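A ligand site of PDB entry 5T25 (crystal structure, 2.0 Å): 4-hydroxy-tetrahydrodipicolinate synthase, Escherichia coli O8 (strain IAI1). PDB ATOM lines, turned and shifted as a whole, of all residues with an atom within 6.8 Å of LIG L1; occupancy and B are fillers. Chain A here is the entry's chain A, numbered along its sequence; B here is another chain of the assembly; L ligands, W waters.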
ATOM      1  N   VAL A  43      -5.327  13.279   2.814  1.00  0.00           N
ATOM      2  CA  VAL A  43      -6.055  13.964   1.742  1.00  0.00           C
ATOM      3  C   VAL A  43      -5.204  15.086   1.126  1.00  0.00           C
ATOM      4  O   VAL A  43      -5.636  16.241   1.026  1.00  0.00           O
ATOM      5  CB  VAL A  43      -7.425  14.478   2.236  1.00  0.00           C
ATOM      6  CG1 VAL A  43      -8.280  14.942   1.063  1.00  0.00           C
ATOM      7  CG2 VAL A  43      -8.168  13.376   2.975  1.00  0.00           C
ATOM      8  N   GLU A  48      -6.466  12.088  -3.381  1.00  0.00           N
ATOM      9  CA  GLU A  48      -7.612  12.463  -4.215  1.00  0.00           C
ATOM     10  C   GLU A  48      -8.455  13.558  -3.571  1.00  0.00           C
ATOM     11  O   GLU A  48      -9.680  13.511  -3.584  1.00  0.00           O
ATOM     12  CB  GLU A  48      -8.449  11.224  -4.554  1.00  0.00           C
ATOM     13  CG  GLU A  48      -7.783  10.316  -5.601  1.00  0.00           C
ATOM     14  CD  GLU A  48      -8.462   8.956  -5.735  1.00  0.00           C
ATOM     15  OE1 GLU A  48      -8.068   8.010  -5.015  1.00  0.00           O
ATOM     16  OE2 GLU A  48      -9.386   8.837  -6.576  1.00  0.00           O
ATOM     17  N   SER A  49      -7.772  14.574  -3.011  1.00  0.00           N
ATOM     18  CA  SER A  49      -8.470  15.724  -2.429  1.00  0.00           C
ATOM     19  C   SER A  49      -9.546  16.295  -3.354  1.00  0.00           C
ATOM     20  O   SER A  49     -10.612  16.715  -2.874  1.00  0.00           O
ATOM     21  CB  SER A  49      -7.451  16.821  -2.080  1.00  0.00           C
ATOM     22  OG  SER A  49      -6.850  17.373  -3.238  1.00  0.00           O
ATOM     23  N   ALA A  50      -9.311  16.307  -4.665  1.00  0.00           N
ATOM     24  CA  ALA A  50     -10.245  16.976  -5.575  1.00  0.00           C
ATOM     25  C   ALA A  50     -11.625  16.326  -5.575  1.00  0.00           C
ATOM     26  O   ALA A  50     -12.650  17.032  -5.666  1.00  0.00           O
ATOM     27  CB  ALA A  50      -9.683  17.001  -7.002  1.00  0.00           C
ATOM     28  N   THR A  51     -11.688  14.992  -5.502  1.00  0.00           N
ATOM     29  CA  THR A  51     -12.933  14.268  -5.734  1.00  0.00           C
ATOM     30  C   THR A  51     -13.634  13.816  -4.455  1.00  0.00           C
ATOM     31  O   THR A  51     -14.617  13.069  -4.529  1.00  0.00           O
ATOM     32  CB  THR A  51     -12.672  13.055  -6.636  1.00  0.00           C
ATOM     33  OG1 THR A  51     -11.636  12.248  -6.057  1.00  0.00           O
ATOM     34  CG2 THR A  51     -12.239  13.507  -8.028  1.00  0.00           C
ATOM     35  N   LEU A  52     -13.180  14.262  -3.284  1.00  0.00           N
ATOM     36  CA  LEU A  52     -13.916  14.090  -2.028  1.00  0.00           C
ATOM     37  C   LEU A  52     -14.603  15.406  -1.717  1.00  0.00           C
ATOM     38  O   LEU A  52     -13.978  16.467  -1.806  1.00  0.00           O
ATOM     39  CB  LEU A  52     -12.977  13.709  -0.880  1.00  0.00           C
ATOM     40  CG  LEU A  52     -12.073  12.483  -1.016  1.00  0.00           C
ATOM     41  CD1 LEU A  52     -11.024  12.397   0.121  1.00  0.00           C
ATOM     42  CD2 LEU A  52     -12.905  11.241  -1.039  1.00  0.00           C
ATOM     43  N   ASN A  53     -15.892  15.351  -1.373  1.00  0.00           N
ATOM     44  CA  ASN A  53     -16.538  16.596  -0.965  1.00  0.00           C
ATOM     45  C   ASN A  53     -16.042  17.000   0.423  1.00  0.00           C
ATOM     46  O   ASN A  53     -15.309  16.272   1.073  1.00  0.00           O
ATOM     47  CB  ASN A  53     -18.074  16.478  -1.037  1.00  0.00           C
ATOM     48  CG  ASN A  53     -18.669  15.506  -0.019  1.00  0.00           C
ATOM     49  OD1 ASN A  53     -18.215  15.398   1.119  1.00  0.00           O
ATOM     50  ND2 ASN A  53     -19.717  14.831  -0.421  1.00  0.00           N
ATOM     51  N   HIS A  54     -16.448  18.202   0.874  1.00  0.00           N
ATOM     52  CA  HIS A  54     -15.870  18.744   2.107  1.00  0.00           C
ATOM     53  C   HIS A  54     -16.108  17.810   3.293  1.00  0.00           C
ATOM     54  O   HIS A  54     -15.213  17.613   4.123  1.00  0.00           O
ATOM     55  CB  HIS A  54     -16.444  20.133   2.382  1.00  0.00           C
ATOM     56  CG  HIS A  54     -15.955  21.179   1.430  1.00  0.00           C
ATOM     57  ND1 HIS A  54     -14.663  21.663   1.457  1.00  0.00           N
ATOM     58  CD2 HIS A  54     -16.575  21.813   0.396  1.00  0.00           C
ATOM     59  CE1 HIS A  54     -14.508  22.554   0.494  1.00  0.00           C
ATOM     60  NE2 HIS A  54     -15.657  22.665  -0.166  1.00  0.00           N
ATOM     61  N   ASP A  55     -17.287  17.187   3.358  1.00  0.00           N
ATOM     62  CA  ASP A  55     -17.594  16.279   4.473  1.00  0.00           C
ATOM     63  C   ASP A  55     -16.818  14.972   4.367  1.00  0.00           C
ATOM     64  O   ASP A  55     -16.323  14.457   5.384  1.00  0.00           O
ATOM     65  CB  ASP A  55     -19.104  16.021   4.523  1.00  0.00           C
ATOM     66  CG  ASP A  55     -19.871  17.197   5.108  1.00  0.00           C
ATOM     67  OD1 ASP A  55     -19.234  18.086   5.693  1.00  0.00           O
ATOM     68  OD2 ASP A  55     -21.111  17.234   4.984  1.00  0.00           O
ATOM     69  N   HIS A  57     -13.925  14.603   2.809  1.00  0.00           N
ATOM     70  CA  HIS A  57     -12.562  15.036   3.080  1.00  0.00           C
ATOM     71  C   HIS A  57     -12.298  15.066   4.580  1.00  0.00           C
ATOM     72  O   HIS A  57     -11.367  14.424   5.083  1.00  0.00           O
ATOM     73  CB  HIS A  57     -12.352  16.411   2.424  1.00  0.00           C
ATOM     74  CG  HIS A  57     -10.962  16.991   2.567  1.00  0.00           C
ATOM     75  ND1 HIS A  57     -10.458  17.899   1.659  1.00  0.00           N
ATOM     76  CD2 HIS A  57     -10.005  16.822   3.502  1.00  0.00           C
ATOM     77  CE1 HIS A  57      -9.236  18.248   2.017  1.00  0.00           C
ATOM     78  NE2 HIS A  57      -8.927  17.617   3.139  1.00  0.00           N
ATOM     79  N   GLY A  79      -5.759  22.558   1.460  1.00  0.00           N
ATOM     80  CA  GLY A  79      -5.650  23.533   0.395  1.00  0.00           C
ATOM     81  C   GLY A  79      -6.979  23.771  -0.295  1.00  0.00           C
ATOM     82  O   GLY A  79      -7.859  22.915  -0.309  1.00  0.00           O
ATOM     83  N   ALA A  80      -7.113  24.966  -0.865  1.00  0.00           N
ATOM     84  CA  ALA A  80      -8.272  25.328  -1.683  1.00  0.00           C
ATOM     85  C   ALA A  80      -7.868  26.488  -2.568  1.00  0.00           C
ATOM     86  O   ALA A  80      -6.953  27.246  -2.239  1.00  0.00           O
ATOM     87  CB  ALA A  80      -9.492  25.675  -0.809  1.00  0.00           C
ATOM     88  N   ASN A  81      -8.558  26.636  -3.703  1.00  0.00           N
ATOM     89  CA  ASN A  81      -8.280  27.770  -4.566  1.00  0.00           C
ATOM     90  C   ASN A  81      -9.185  28.967  -4.280  1.00  0.00           C
ATOM     91  O   ASN A  81      -9.028  30.017  -4.910  1.00  0.00           O
ATOM     92  CB  ASN A  81      -8.362  27.356  -6.048  1.00  0.00           C
ATOM     93  CG  ASN A  81      -9.723  26.827  -6.463  1.00  0.00           C
ATOM     94  OD1 ASN A  81     -10.628  26.677  -5.656  1.00  0.00           O
ATOM     95  ND2 ASN A  81      -9.855  26.544  -7.759  1.00  0.00           N
ATOM     96  N   GLU A  85     -12.870  28.894   1.282  1.00  0.00           N
ATOM     97  CA  GLU A  85     -12.887  27.431   1.394  1.00  0.00           C
ATOM     98  C   GLU A  85     -11.723  26.920   2.222  1.00  0.00           C
ATOM     99  O   GLU A  85     -11.870  25.980   3.016  1.00  0.00           O
ATOM    100  CB  GLU A  85     -12.823  26.812   0.011  1.00  0.00           C
ATOM    101  CG  GLU A  85     -14.117  26.444  -0.602  1.00  0.00           C
ATOM    102  CD  GLU A  85     -13.885  25.729  -1.913  1.00  0.00           C
ATOM    103  OE1 GLU A  85     -14.053  26.363  -2.976  1.00  0.00           O
ATOM    104  OE2 GLU A  85     -13.517  24.535  -1.884  1.00  0.00           O
ATOM    105  N   LEU A  89     -12.077  24.818   5.691  1.00  0.00           N
ATOM    106  CA  LEU A  89     -11.483  23.499   5.844  1.00  0.00           C
ATOM    107  C   LEU A  89     -10.499  23.472   7.016  1.00  0.00           C
ATOM    108  O   LEU A  89     -10.485  22.521   7.803  1.00  0.00           O
ATOM    109  CB  LEU A  89     -10.766  23.123   4.544  1.00  0.00           C
ATOM    110  CG  LEU A  89     -10.621  21.698   4.002  1.00  0.00           C
ATOM    111  CD1 LEU A  89     -11.823  20.816   4.304  1.00  0.00           C
ATOM    112  CD2 LEU A  89     -10.391  21.803   2.503  1.00  0.00           C
ATOM    113  N   TYR A 107      -5.250  26.810  -7.288  1.00  0.00           N
ATOM    114  CA  TYR A 107      -5.074  26.238  -8.615  1.00  0.00           C
ATOM    115  C   TYR A 107      -6.158  26.758  -9.540  1.00  0.00           C
ATOM    116  O   TYR A 107      -7.238  27.145  -9.087  1.00  0.00           O
ATOM    117  CB  TYR A 107      -5.106  24.713  -8.575  1.00  0.00           C
ATOM    118  CG  TYR A 107      -6.058  24.149  -7.530  1.00  0.00           C
ATOM    119  CD1 TYR A 107      -7.411  23.967  -7.812  1.00  0.00           C
ATOM    120  CD2 TYR A 107      -5.608  23.817  -6.253  1.00  0.00           C
ATOM    121  CE1 TYR A 107      -8.287  23.441  -6.851  1.00  0.00           C
ATOM    122  CE2 TYR A 107      -6.462  23.289  -5.295  1.00  0.00           C
ATOM    123  CZ  TYR A 107      -7.802  23.121  -5.593  1.00  0.00           C
ATOM    124  OH  TYR A 107      -8.669  22.605  -4.635  1.00  0.00           O
ATOM    125  N   ALA B  80     -15.849  21.321 -13.601  1.00  0.00           N
ATOM    126  CA  ALA B  80     -15.399  20.904 -12.278  1.00  0.00           C
ATOM    127  C   ALA B  80     -14.279  19.899 -12.455  1.00  0.00           C
ATOM    128  O   ALA B  80     -14.179  19.236 -13.494  1.00  0.00           O
ATOM    129  CB  ALA B  80     -16.545  20.299 -11.442  1.00  0.00           C
ATOM    130  N   ASN B  81     -13.415  19.793 -11.453  1.00  0.00           N
ATOM    131  CA  ASN B  81     -12.359  18.805 -11.558  1.00  0.00           C
ATOM    132  C   ASN B  81     -12.746  17.456 -10.941  1.00  0.00           C
ATOM    133  O   ASN B  81     -11.955  16.514 -10.975  1.00  0.00           O
ATOM    134  CB  ASN B  81     -11.048  19.345 -10.973  1.00  0.00           C
ATOM    135  CG  ASN B  81     -11.131  19.637  -9.489  1.00  0.00           C
ATOM    136  OD1 ASN B  81     -12.207  19.635  -8.906  1.00  0.00           O
ATOM    137  ND2 ASN B  81      -9.986  19.925  -8.880  1.00  0.00           N
ATOM    138  N   ALA B  82     -13.959  17.353 -10.403  1.00  0.00           N
ATOM    139  CA  ALA B  82     -14.544  16.080 -10.004  1.00  0.00           C
ATOM    140  C   ALA B  82     -15.763  15.830 -10.884  1.00  0.00           C
ATOM    141  O   ALA B  82     -16.641  16.691 -10.982  1.00  0.00           O
ATOM    142  CB  ALA B  82     -14.929  16.079  -8.534  1.00  0.00           C
ATOM    143  N   GLU B  85     -19.084  16.408  -9.269  1.00  0.00           N
ATOM    144  CA  GLU B  85     -19.411  17.825  -9.142  1.00  0.00           C
ATOM    145  C   GLU B  85     -19.905  18.391 -10.462  1.00  0.00           C
ATOM    146  O   GLU B  85     -20.841  19.206 -10.489  1.00  0.00           O
ATOM    147  CB  GLU B  85     -18.184  18.614  -8.682  1.00  0.00           C
ATOM    148  CG  GLU B  85     -17.968  18.658  -7.183  1.00  0.00           C
ATOM    149  CD  GLU B  85     -16.594  19.236  -6.835  1.00  0.00           C
ATOM    150  OE1 GLU B  85     -15.960  19.806  -7.726  1.00  0.00           O
ATOM    151  OE2 GLU B  85     -16.159  19.133  -5.671  1.00  0.00           O
ATOM    152  N   TYR B 107      -8.991  20.509 -13.555  1.00  0.00           N
ATOM    153  CA  TYR B 107      -7.765  21.198 -13.187  1.00  0.00           C
ATOM    154  C   TYR B 107      -7.188  20.576 -11.913  1.00  0.00           C
ATOM    155  O   TYR B 107      -7.930  20.030 -11.081  1.00  0.00           O
ATOM    156  CB  TYR B 107      -8.025  22.693 -12.979  1.00  0.00           C
ATOM    157  CG  TYR B 107      -9.394  22.970 -12.378  1.00  0.00           C
ATOM    158  CD1 TYR B 107      -9.600  22.889 -11.010  1.00  0.00           C
ATOM    159  CD2 TYR B 107     -10.486  23.304 -13.187  1.00  0.00           C
ATOM    160  CE1 TYR B 107     -10.853  23.138 -10.455  1.00  0.00           C
ATOM    161  CE2 TYR B 107     -11.730  23.553 -12.636  1.00  0.00           C
ATOM    162  CZ  TYR B 107     -11.914  23.471 -11.271  1.00  0.00           C
ATOM    163  OH  TYR B 107     -13.153  23.702 -10.693  1.00  0.00           O
ATOM    164  N   TYR B 108      -5.859  20.639 -11.802  1.00  0.00           N
ATOM    165  CA  TYR B 108      -5.088  20.264 -10.620  1.00  0.00           C
ATOM    166  C   TYR B 108      -4.870  18.761 -10.473  1.00  0.00           C
ATOM    167  O   TYR B 108      -3.779  18.353 -10.081  1.00  0.00           O
ATOM    168  CB  TYR B 108      -5.730  20.843  -9.363  1.00  0.00           C
ATOM    169  CG  TYR B 108      -5.007  20.537  -8.078  1.00  0.00           C
ATOM    170  CD1 TYR B 108      -3.723  21.010  -7.854  1.00  0.00           C
ATOM    171  CD2 TYR B 108      -5.631  19.801  -7.076  1.00  0.00           C
ATOM    172  CE1 TYR B 108      -3.061  20.756  -6.662  1.00  0.00           C
ATOM    173  CE2 TYR B 108      -4.986  19.535  -5.876  1.00  0.00           C
ATOM    174  CZ  TYR B 108      -3.687  20.016  -5.684  1.00  0.00           C
ATOM    175  OH  TYR B 108      -3.024  19.771  -4.489  1.00  0.00           O
HETATM  176  N1  LIG L   1     -13.172  19.645  -6.402  1.00  0.00           N
HETATM  177  C1  LIG L   1     -12.954  20.925  -5.744  1.00  0.00           C
HETATM  178  C2  LIG L   1     -11.473  21.242  -5.621  1.00  0.00           C
HETATM  179  O1  LIG L   1     -11.070  22.291  -5.131  1.00  0.00           O
HETATM  180  C3  LIG L   1     -13.597  20.946  -4.348  1.00  0.00           C
HETATM  181  C4  LIG L   1     -12.819  20.160  -3.304  1.00  0.00           C
HETATM  182  C5  LIG L   1     -13.628  19.951  -2.038  1.00  0.00           C
HETATM  183  C6  LIG L   1     -12.742  19.642  -0.833  1.00  0.00           C
HETATM  184  N2  LIG L   1     -11.954  18.390  -0.990  1.00  0.00           N
HETATM  185  O2  LIG L   1     -10.638  20.448  -6.027  1.00  0.00           O
HETATM  186  N1  LG2 L   2     -13.307  26.239  -5.489  1.00  0.00           N
HETATM  187  C1  LG2 L   2     -13.733  24.965  -6.063  1.00  0.00           C
HETATM  188  C2  LG2 L   2     -13.321  24.866  -7.521  1.00  0.00           C
HETATM  189  O1  LG2 L   2     -13.464  23.809  -8.142  1.00  0.00           O
HETATM  190  C3  LG2 L   2     -15.251  24.778  -5.923  1.00  0.00           C
HETATM  191  C4  LG2 L   2     -16.090  25.443  -7.005  1.00  0.00           C
HETATM  192  C5  LG2 L   2     -17.552  25.508  -6.585  1.00  0.00           C
HETATM  193  C6  LG2 L   2     -18.468  25.897  -7.733  1.00  0.00           C
HETATM  194  N2  LG2 L   2     -18.078  27.205  -8.352  1.00  0.00           N
HETATM  195  O2  LG2 L   2     -12.809  25.820  -8.100  1.00  0.00           O
HETATM  196  O   HOH W   1      -8.275  19.580  -4.528  1.00  0.00           O
HETATM  197  O   HOH W   2      -9.552  19.739  -1.938  1.00  0.00           O
HETATM  198  O   HOH W   3     -11.134  24.156  -3.319  1.00  0.00           O
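The side-chain hydroxyl of Tyr 107 of chain A lies within hydrogen-bond range of an oxygen (O1) of LIG L1, 2.5 Å away.
A nitrogen (N1) of LIG L1 lies within hydrogen-bond range of the side-chain amide oxygen (OD1) of Asn 81 of chain B, 2.7 Å away.
A nitrogen (N1) of LIG L1 sits at hydrogen-bond distance from the backbone carbonyl oxygen (O) of Ala 50.
The backbone carbonyl oxygen (O) of Ser 49 lies within hydrogen-bond range of a nitrogen (N2) of LIG L1 (2.9 Å).
O of Leu 52 is in hydrogen-bond range of N2 of LIG L1, at 2.9 Å.
A ring nitrogen (ND1) of His 57 is in hydrogen-bond range of a nitrogen (N2) of LIG L1, at 3.1 Å.
The side-chain carboxylate (OE1) of Glu 85 of chain B is in salt-bridge range of a nitrogen (N1) of LIG L1 (3.1 Å).
The side-chain carboxylate of Glu 85 of chain A lies within salt-bridge range of a nitrogen (N1) of LG2 L2.
A nitrogen (N1) of LG2 L2 is in hydrogen-bond range of the side-chain amide oxygen (OD1) of Asn 81 of chain A (2.7 Å).
An oxygen (O1) of LG2 L2 is in hydrogen-bond range of the side-chain hydroxyl (OH) of Tyr 107 of chain B (2.6 Å).
The side-chain amide nitrogen (ND2) of Asn 81 of chain A lies within hydrogen-bond range of the backbone carbonyl oxygen (O) of Tyr 107 of chain A.
The side-chain amide nitrogen (ND2) of Asn 81 of chain B sits at hydrogen-bond distance from the backbone carbonyl oxygen (O) of Tyr 107 of chain B, at 3.0 Å.
The side-chain carboxylate (OE2) of Glu 85 of chain A lies close to a ring nitrogen (NE2) of His 54 (3.3 Å).
His 54 touches LIG L1.
Hydrophobic or aromatic side chains that line LIG L1: Ala 50, His 54, His 57 and Tyr 107 of chain A.
Eight residues have an atom within 4 Å of LIG L1: Ser 49, Ala 50, Leu 52, His 54, His 57, Tyr 107 of chain A, Asn 81 of chain B and Glu 85 of chain B.
Along chain A the residues within 4 Å of LIG L1 span positions 49 to 107.
Water W3 lies within hydrogen-bond range of an oxygen (O1) of LIG L1 (2.6 Å), the side-chain carboxylate (OE2) of Glu 85 of chain A (2.8 Å), the side-chain hydroxyl (OH) of Tyr 107 of chain A (3.2 Å) and the side-chain amide oxygen (OD1) of Asn 81 of chain A (3.5 Å).
Water W2 lies within hydrogen-bond range of N2 of LIG L1 (2.9 Å) and O of Ser 49 (3.3 Å).
Water W1 lies within hydrogen-bond range of the side-chain hydroxyl (OG) of Ser 49 (2.9 Å), an oxygen (O2) of LIG L1 (2.9 Å), the side-chain hydroxyl (OH) of Tyr 107 of chain A (3.1 Å) and the backbone NH (N) of Ala 50 (3.4 Å).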
